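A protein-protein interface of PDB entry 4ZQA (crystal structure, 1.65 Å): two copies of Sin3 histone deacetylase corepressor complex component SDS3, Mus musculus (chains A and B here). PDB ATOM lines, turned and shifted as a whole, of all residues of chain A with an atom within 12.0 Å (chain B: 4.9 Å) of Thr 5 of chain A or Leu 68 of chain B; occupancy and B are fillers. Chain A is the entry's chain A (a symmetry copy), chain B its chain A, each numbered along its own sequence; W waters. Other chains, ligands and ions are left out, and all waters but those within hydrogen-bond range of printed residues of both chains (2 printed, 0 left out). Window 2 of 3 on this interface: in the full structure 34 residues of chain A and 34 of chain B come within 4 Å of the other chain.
O of Ser 1 of chain A lies within hydrogen-bond range of NZ of Lys 71 of chain B (3.4 Å).
NZ of Lys 71 of chain B sits at hydrogen-bond distance from OG1 of Thr 5 of chain A (3.1 Å).
Asn 2 of chain A touches Lys 71 of chain B.
Thr 5 of chain A touches Leu 64 of chain B (CG2 to CD1, 3.6 Å).
Glu 67 of chain B touches Thr 5 of chain A (OE1 to OG1, 3.8 Å).
CG2 of Thr 5 of chain A touches CD2 of Leu 68 of chain B, 3.97 Å away.
Tyr 9 of chain A touches Leu 64 of chain B.
Printed residues of chain B within 4 Å of Ser 1 of chain A: Lys 71.
Of the printed residues of chain B, Asn 2 of chain A touches Lys 71.
Thr 5 of chain A touches just these residues of chain B: Leu 64, Glu 67, Leu 68 and Lys 71.
Printed residues of chain B within 4 Å of Tyr 9 of chain A: Leu 64.
Of the printed residues of chain A, Leu 64 of chain B touches Thr 5 (3.6 Å) and Tyr 9 (3.8 Å).
No residue of chain A comes within 4 Å of Ile 65 of chain B.
Ala 66 of chain B touches none of the printed residues of chain A.
Of chain A, only Thr 5 (3.8 Å) comes within 4 Å of Glu 67 of chain B.
Leu 68 of chain B touches just one residue of chain A: Thr 5 (3.97 Å).
The nearest residue of chain A that does not touch Leu 68 of chain B is Asn 2 of chain A (4.2 Å).
The nearest printed residue of chain B that does not touch Tyr 9 of chain A is Ile 65 of chain B (6.9 Å).
Along chain B the printed residues that touch a printed residue of chain A span positions 64 to 71.
Of the 14 printed residues of chain A, 4 touch a printed residue of chain B.
Printed residues of chain A that touch a printed residue of chain B: Ser 1, Asn 2, Thr 5 and Tyr 9.
Hydrophobic or aromatic side chains of chain A that line the printed part of chain B: Tyr 9.
Among the printed residues, 7 pairs touch across the chains.
No position is printed for both chains.
Of the 7 pairs that touch across the chains among the printed residues, none has its exchanged pair printed and touching as well.
Water W2 lies within hydrogen-bond range of the backbone carbonyl oxygen (O) of Ser 1 of chain A, the side-chain hydroxyl (OG1) of Thr 5 of chain A and the side-chain amino group (NZ) of Lys 71 of chain B.
Water W1 lies within hydrogen-bond range of OE2 of Glu 67 of chain B (3.3 Å) and NH1 of Arg 12 of chain A (3.4 Å).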
ATOM      1  N   SER A   1       5.733  -8.811   0.271  1.00  0.00           N
ATOM      2  CA  SER A   1       5.497 -10.280   0.122  1.00  0.00           C
ATOM      3  C   SER A   1       6.515 -11.023   0.984  1.00  0.00           C
ATOM      4  O   SER A   1       6.141 -11.666   1.978  1.00  0.00           O
ATOM      5  CB  SER A   1       5.576 -10.702  -1.356  1.00  0.00           C
ATOM      6  OG  SER A   1       5.016 -11.997  -1.567  1.00  0.00           O
ATOM      7  N   ASN A   2       7.796 -10.929   0.610  1.00  0.00           N
ATOM      8  CA  ASN A   2       8.905 -11.262   1.537  1.00  0.00           C
ATOM      9  C   ASN A   2       9.470 -10.063   2.305  1.00  0.00           C
ATOM     10  O   ASN A   2      10.365 -10.237   3.131  1.00  0.00           O
ATOM     11  CB  ASN A   2      10.043 -12.080   0.846  1.00  0.00           C
ATOM     12  CG  ASN A   2      10.780 -11.300  -0.269  1.00  0.00           C
ATOM     13  OD1 ASN A   2      10.670 -10.064  -0.367  1.00  0.00           O
ATOM     14  ND2 ASN A   2      11.540 -12.041  -1.140  1.00  0.00           N
ATOM     15  N   ALA A   3       8.939  -8.866   2.051  1.00  0.00           N
ATOM     16  CA  ALA A   3       9.437  -7.625   2.646  1.00  0.00           C
ATOM     17  C   ALA A   3       9.548  -7.660   4.198  1.00  0.00           C
ATOM     18  O   ALA A   3      10.556  -7.227   4.764  1.00  0.00           O
ATOM     19  CB  ALA A   3       8.567  -6.448   2.191  1.00  0.00           C
ATOM     20  N   GLY A   4       8.524  -8.189   4.870  1.00  0.00           N
ATOM     21  CA  GLY A   4       8.509  -8.257   6.344  1.00  0.00           C
ATOM     22  C   GLY A   4       9.521  -9.255   6.908  1.00  0.00           C
ATOM     23  O   GLY A   4      10.204  -8.989   7.911  1.00  0.00           O
ATOM     24  N   THR A   5       9.605 -10.421   6.276  1.00  0.00           N
ATOM     25  CA  THR A   5      10.632 -11.421   6.618  1.00  0.00           C
ATOM     26  C   THR A   5      12.036 -10.845   6.453  1.00  0.00           C
ATOM     27  O   THR A   5      12.898 -11.005   7.346  1.00  0.00           O
ATOM     28  CB  THR A   5      10.447 -12.695   5.761  1.00  0.00           C
ATOM     29  OG1 THR A   5       9.149 -13.262   6.045  1.00  0.00           O
ATOM     30  CG2 THR A   5      11.561 -13.760   5.996  1.00  0.00           C
ATOM     31  N   LEU A   6      12.271 -10.133   5.355  1.00  0.00           N
ATOM     32  CA  LEU A   6      13.610  -9.585   5.112  1.00  0.00           C
ATOM     33  C   LEU A   6      13.908  -8.470   6.111  1.00  0.00           C
ATOM     34  O   LEU A   6      15.030  -8.368   6.597  1.00  0.00           O
ATOM     35  CB  LEU A   6      13.797  -9.149   3.666  1.00  0.00           C
ATOM     36  CG  LEU A   6      13.663 -10.273   2.595  1.00  0.00           C
ATOM     37  CD1 LEU A   6      13.900  -9.717   1.187  1.00  0.00           C
ATOM     38  CD2 LEU A   6      14.595 -11.445   2.848  1.00  0.00           C
ATOM     39  N   GLN A   7      12.873  -7.685   6.439  1.00  0.00           N
ATOM     40  CA  GLN A   7      12.916  -6.649   7.462  1.00  0.00           C
ATOM     41  C   GLN A   7      13.272  -7.143   8.859  1.00  0.00           C
ATOM     42  O   GLN A   7      14.187  -6.590   9.506  1.00  0.00           O
ATOM     43  CB  GLN A   7      11.556  -5.914   7.497  1.00  0.00           C
ATOM     44  CG  GLN A   7      11.463  -4.811   6.472  1.00  0.00           C
ATOM     45  CD  GLN A   7      12.606  -3.821   6.621  1.00  0.00           C
ATOM     46  OE1 GLN A   7      12.737  -3.161   7.664  1.00  0.00           O
ATOM     47  NE2 GLN A   7      13.458  -3.729   5.588  1.00  0.00           N
ATOM     48  N   GLU A   8      12.572  -8.176   9.323  1.00  0.00           N
ATOM     49  CA  GLU A   8      12.915  -8.842  10.584  1.00  0.00           C
ATOM     50  C   GLU A   8      14.373  -9.281  10.560  1.00  0.00           C
ATOM     51  O   GLU A   8      15.077  -9.132  11.552  1.00  0.00           O
ATOM     52  CB  GLU A   8      12.071 -10.110  10.829  1.00  0.00           C
ATOM     53  CG  GLU A   8      10.940  -9.971  11.808  1.00  0.00           C
ATOM     54  CD  GLU A   8      11.392  -9.705  13.232  1.00  0.00           C
ATOM     55  OE1 GLU A   8      12.509 -10.140  13.597  1.00  0.00           O
ATOM     56  OE2 GLU A   8      10.613  -9.068  13.982  1.00  0.00           O
ATOM     57  N   TYR A   9      14.809  -9.874   9.437  1.00  0.00           N
ATOM     58  CA  TYR A   9      16.191 -10.406   9.354  1.00  0.00           C
ATOM     59  C   TYR A   9      17.238  -9.305   9.557  1.00  0.00           C
ATOM     60  O   TYR A   9      18.175  -9.452  10.351  1.00  0.00           O
ATOM     61  CB  TYR A   9      16.379 -11.087   7.991  1.00  0.00           C
ATOM     62  CG  TYR A   9      17.795 -11.568   7.717  1.00  0.00           C
ATOM     63  CD1 TYR A   9      18.266 -12.753   8.269  1.00  0.00           C
ATOM     64  CD2 TYR A   9      18.653 -10.808   6.950  1.00  0.00           C
ATOM     65  CE1 TYR A   9      19.574 -13.167   8.032  1.00  0.00           C
ATOM     66  CE2 TYR A   9      19.967 -11.218   6.683  1.00  0.00           C
ATOM     67  CZ  TYR A   9      20.426 -12.392   7.235  1.00  0.00           C
ATOM     68  OH  TYR A   9      21.701 -12.831   6.967  1.00  0.00           O
ATOM     69  N   GLN A  10      17.072  -8.196   8.830  1.00  0.00           N
ATOM     70  CA  GLN A  10      17.971  -7.068   8.933  1.00  0.00           C
ATOM     71  C   GLN A  10      17.956  -6.476  10.359  1.00  0.00           C
ATOM     72  O   GLN A  10      18.998  -6.095  10.854  1.00  0.00           O
ATOM     73  CB  GLN A  10      17.669  -6.001   7.878  1.00  0.00           C
ATOM     74  CG  GLN A  10      17.873  -6.516   6.450  1.00  0.00           C
ATOM     75  CD  GLN A  10      18.253  -5.428   5.451  1.00  0.00           C
ATOM     76  OE1 GLN A  10      17.431  -4.577   5.078  1.00  0.00           O
ATOM     77  NE2 GLN A  10      19.498  -5.474   4.983  1.00  0.00           N
ATOM     78  N   LYS A  11      16.783  -6.422  10.997  1.00  0.00           N
ATOM     79  CA  LYS A  11      16.681  -5.956  12.394  1.00  0.00           C
ATOM     80  C   LYS A  11      17.544  -6.847  13.273  1.00  0.00           C
ATOM     81  O   LYS A  11      18.322  -6.381  14.109  1.00  0.00           O
ATOM     82  CB  LYS A  11      15.214  -6.014  12.876  1.00  0.00           C
ATOM     83  CG  LYS A  11      14.949  -5.383  14.239  1.00  0.00           C
ATOM     84  CD  LYS A  11      13.649  -5.893  14.882  1.00  0.00           C
ATOM     85  CE  LYS A  11      12.510  -6.027  13.884  1.00  0.00           C
ATOM     86  NZ  LYS A  11      11.213  -6.402  14.530  1.00  0.00           N
ATOM     87  N   ARG A  12      17.399  -8.144  13.092  1.00  0.00           N
ATOM     88  CA  ARG A  12      18.088  -9.091  13.945  1.00  0.00           C
ATOM     89  C   ARG A  12      19.595  -9.075  13.690  1.00  0.00           C
ATOM     90  O   ARG A  12      20.382  -9.227  14.618  1.00  0.00           O
ATOM     91  CB  ARG A  12      17.510 -10.501  13.764  1.00  0.00           C
ATOM     92  CG  ARG A  12      16.113 -10.636  14.308  1.00  0.00           C
ATOM     93  CD  ARG A  12      15.524 -11.996  13.999  1.00  0.00           C
ATOM     94  NE  ARG A  12      14.247 -12.182  14.688  1.00  0.00           N
ATOM     95  CZ  ARG A  12      13.336 -13.102  14.386  1.00  0.00           C
ATOM     96  NH1 ARG A  12      13.509 -13.935  13.366  1.00  0.00           N
ATOM     97  NH2 ARG A  12      12.226 -13.162  15.095  1.00  0.00           N
ATOM     98  N   MET A  13      19.993  -8.906  12.442  1.00  0.00           N
ATOM     99  CA  MET A  13      21.428  -8.779  12.113  1.00  0.00           C
ATOM    100  C   MET A  13      22.048  -7.572  12.819  1.00  0.00           C
ATOM    101  O   MET A  13      23.108  -7.690  13.408  1.00  0.00           O
ATOM    102  CB  MET A  13      21.618  -8.655  10.605  1.00  0.00           C
ATOM    103  CG  MET A  13      21.368  -9.983   9.908  1.00  0.00           C
ATOM    104  SD  MET A  13      22.769 -11.084  10.195  1.00  0.00           S
ATOM    105  CE  MET A  13      24.027 -10.363   9.101  1.00  0.00           C
ATOM    106  N   LYS A  14      21.378  -6.417  12.749  1.00  0.00           N
ATOM    107  CA  LYS A  14      21.812  -5.207  13.469  1.00  0.00           C
ATOM    108  C   LYS A  14      21.942  -5.448  15.001  1.00  0.00           C
ATOM    109  O   LYS A  14      22.912  -4.968  15.621  1.00  0.00           O
ATOM    110  CB  LYS A  14      20.858  -4.029  13.140  1.00  0.00           C
ATOM    111  CG  LYS A  14      21.219  -2.727  13.804  1.00  0.00           C
ATOM    112  CD  LYS A  14      20.350  -1.558  13.329  1.00  0.00           C
ATOM    113  CE  LYS A  14      20.324  -0.425  14.360  1.00  0.00           C
ATOM    114  NZ  LYS A  14      21.663  -0.161  14.985  1.00  0.00           N
ATOM    115  N   LEU B  64      16.784 -17.966   7.780  1.00  0.00           N
ATOM    116  CA  LEU B  64      16.129 -17.160   6.737  1.00  0.00           C
ATOM    117  C   LEU B  64      15.818 -17.995   5.471  1.00  0.00           C
ATOM    118  O   LEU B  64      14.716 -17.944   4.924  1.00  0.00           O
ATOM    119  CB  LEU B  64      16.977 -15.953   6.367  1.00  0.00           C
ATOM    120  CG  LEU B  64      16.459 -15.096   5.211  1.00  0.00           C
ATOM    121  CD1 LEU B  64      15.084 -14.483   5.538  1.00  0.00           C
ATOM    122  CD2 LEU B  64      17.445 -14.034   4.783  1.00  0.00           C
ATOM    123  N   ILE B  65      16.810 -18.772   5.036  1.00  0.00           N
ATOM    124  CA  ILE B  65      16.663 -19.696   3.904  1.00  0.00           C
ATOM    125  C   ILE B  65      15.524 -20.682   4.160  1.00  0.00           C
ATOM    126  O   ILE B  65      14.648 -20.821   3.318  1.00  0.00           O
ATOM    127  CB  ILE B  65      17.989 -20.463   3.606  1.00  0.00           C
ATOM    128  CG1 ILE B  65      19.065 -19.504   3.095  1.00  0.00           C
ATOM    129  CG2 ILE B  65      17.787 -21.584   2.564  1.00  0.00           C
ATOM    130  CD1 ILE B  65      20.496 -20.034   3.181  1.00  0.00           C
ATOM    131  N   ALA B  66      15.508 -21.332   5.320  1.00  0.00           N
ATOM    132  CA  ALA B  66      14.411 -22.221   5.673  1.00  0.00           C
ATOM    133  C   ALA B  66      13.030 -21.497   5.735  1.00  0.00           C
ATOM    134  O   ALA B  66      12.010 -22.032   5.249  1.00  0.00           O
ATOM    135  CB  ALA B  66      14.725 -22.918   6.977  1.00  0.00           C
ATOM    136  N   GLU B  67      13.013 -20.279   6.287  1.00  0.00           N
ATOM    137  CA  GLU B  67      11.775 -19.474   6.405  1.00  0.00           C
ATOM    138  C   GLU B  67      11.217 -19.061   5.047  1.00  0.00           C
ATOM    139  O   GLU B  67      10.000 -19.139   4.805  1.00  0.00           O
ATOM    140  CB  GLU B  67      11.984 -18.221   7.267  1.00  0.00           C
ATOM    141  CG  GLU B  67      10.679 -17.452   7.524  1.00  0.00           C
ATOM    142  CD  GLU B  67      10.699 -16.504   8.733  1.00  0.00           C
ATOM    143  OE1 GLU B  67       9.685 -15.766   8.896  1.00  0.00           O
ATOM    144  OE2 GLU B  67      11.695 -16.488   9.516  1.00  0.00           O
ATOM    145  N   LEU B  68      12.093 -18.626   4.154  1.00  0.00           N
ATOM    146  CA  LEU B  68      11.661 -18.341   2.780  1.00  0.00           C
ATOM    147  C   LEU B  68      11.083 -19.563   2.080  1.00  0.00           C
ATOM    148  O   LEU B  68      10.058 -19.440   1.412  1.00  0.00           O
ATOM    149  CB  LEU B  68      12.792 -17.733   1.953  1.00  0.00           C
ATOM    150  CG  LEU B  68      13.307 -16.353   2.420  1.00  0.00           C
ATOM    151  CD1 LEU B  68      14.500 -15.902   1.594  1.00  0.00           C
ATOM    152  CD2 LEU B  68      12.225 -15.275   2.383  1.00  0.00           C
ATOM    153  N   GLU B  69      11.692 -20.738   2.240  1.00  0.00           N
ATOM    154  CA  GLU B  69      11.068 -21.968   1.707  1.00  0.00           C
ATOM    155  C   GLU B  69       9.693 -22.276   2.366  1.00  0.00           C
ATOM    156  O   GLU B  69       8.748 -22.626   1.687  1.00  0.00           O
ATOM    157  CB  GLU B  69      12.000 -23.187   1.840  1.00  0.00           C
ATOM    158  CG  GLU B  69      11.650 -24.339   0.879  1.00  0.00           C
ATOM    159  CD  GLU B  69      12.121 -24.092  -0.557  1.00  0.00           C
ATOM    160  OE1 GLU B  69      13.062 -23.282  -0.772  1.00  0.00           O
ATOM    161  OE2 GLU B  69      11.555 -24.721  -1.480  1.00  0.00           O
ATOM    162  N   GLU B  70       9.595 -22.132   3.688  1.00  0.00           N
ATOM    163  CA  GLU B  70       8.359 -22.357   4.411  1.00  0.00           C
ATOM    164  C   GLU B  70       7.220 -21.397   3.986  1.00  0.00           C
ATOM    165  O   GLU B  70       6.058 -21.822   3.840  1.00  0.00           O
ATOM    166  CB  GLU B  70       8.604 -22.276   5.928  1.00  0.00           C
ATOM    167  CG  GLU B  70       7.343 -22.473   6.764  1.00  0.00           C
ATOM    168  CD  GLU B  70       6.619 -23.798   6.484  1.00  0.00           C
ATOM    169  OE1 GLU B  70       7.292 -24.813   6.162  1.00  0.00           O
ATOM    170  OE2 GLU B  70       5.365 -23.830   6.588  1.00  0.00           O
ATOM    171  N   LYS B  71       7.548 -20.119   3.784  1.00  0.00           N
ATOM    172  CA  LYS B  71       6.536 -19.146   3.405  1.00  0.00           C
ATOM    173  C   LYS B  71       5.986 -19.476   2.015  1.00  0.00           C
ATOM    174  O   LYS B  71       4.785 -19.351   1.757  1.00  0.00           O
ATOM    175  CB  LYS B  71       7.102 -17.748   3.412  1.00  0.00           C
ATOM    176  CG  LYS B  71       6.006 -16.684   3.440  1.00  0.00           C
ATOM    177  CD  LYS B  71       6.532 -15.327   3.019  1.00  0.00           C
ATOM    178  CE  LYS B  71       7.803 -14.950   3.772  1.00  0.00           C
ATOM    179  NZ  LYS B  71       8.489 -13.863   3.050  1.00  0.00           N
ATOM    180  N   LYS B  72       6.868 -19.931   1.131  1.00  0.00           N
ATOM    181  CA  LYS B  72       6.448 -20.455  -0.180  1.00  0.00           C
ATOM    182  C   LYS B  72       5.284 -21.451  -0.051  1.00  0.00           C
ATOM    183  O   LYS B  72       4.248 -21.338  -0.746  1.00  0.00           O
ATOM    184  CB  LYS B  72       7.650 -21.132  -0.870  1.00  0.00           C
ATOM    185  CG  LYS B  72       7.546 -21.332  -2.373  1.00  0.00           C
ATOM    186  CD  LYS B  72       8.776 -22.065  -2.919  1.00  0.00           C
ATOM    187  CE  LYS B  72      10.096 -21.438  -2.452  1.00  0.00           C
ATOM    188  NZ  LYS B  72      11.300 -21.767  -3.294  1.00  0.00           N
HETATM  189  O   HOH W   1      11.016 -13.638  11.082  1.00  0.00           O
HETATM  190  O   HOH W   2       7.205 -11.520   4.611  1.00  0.00           O
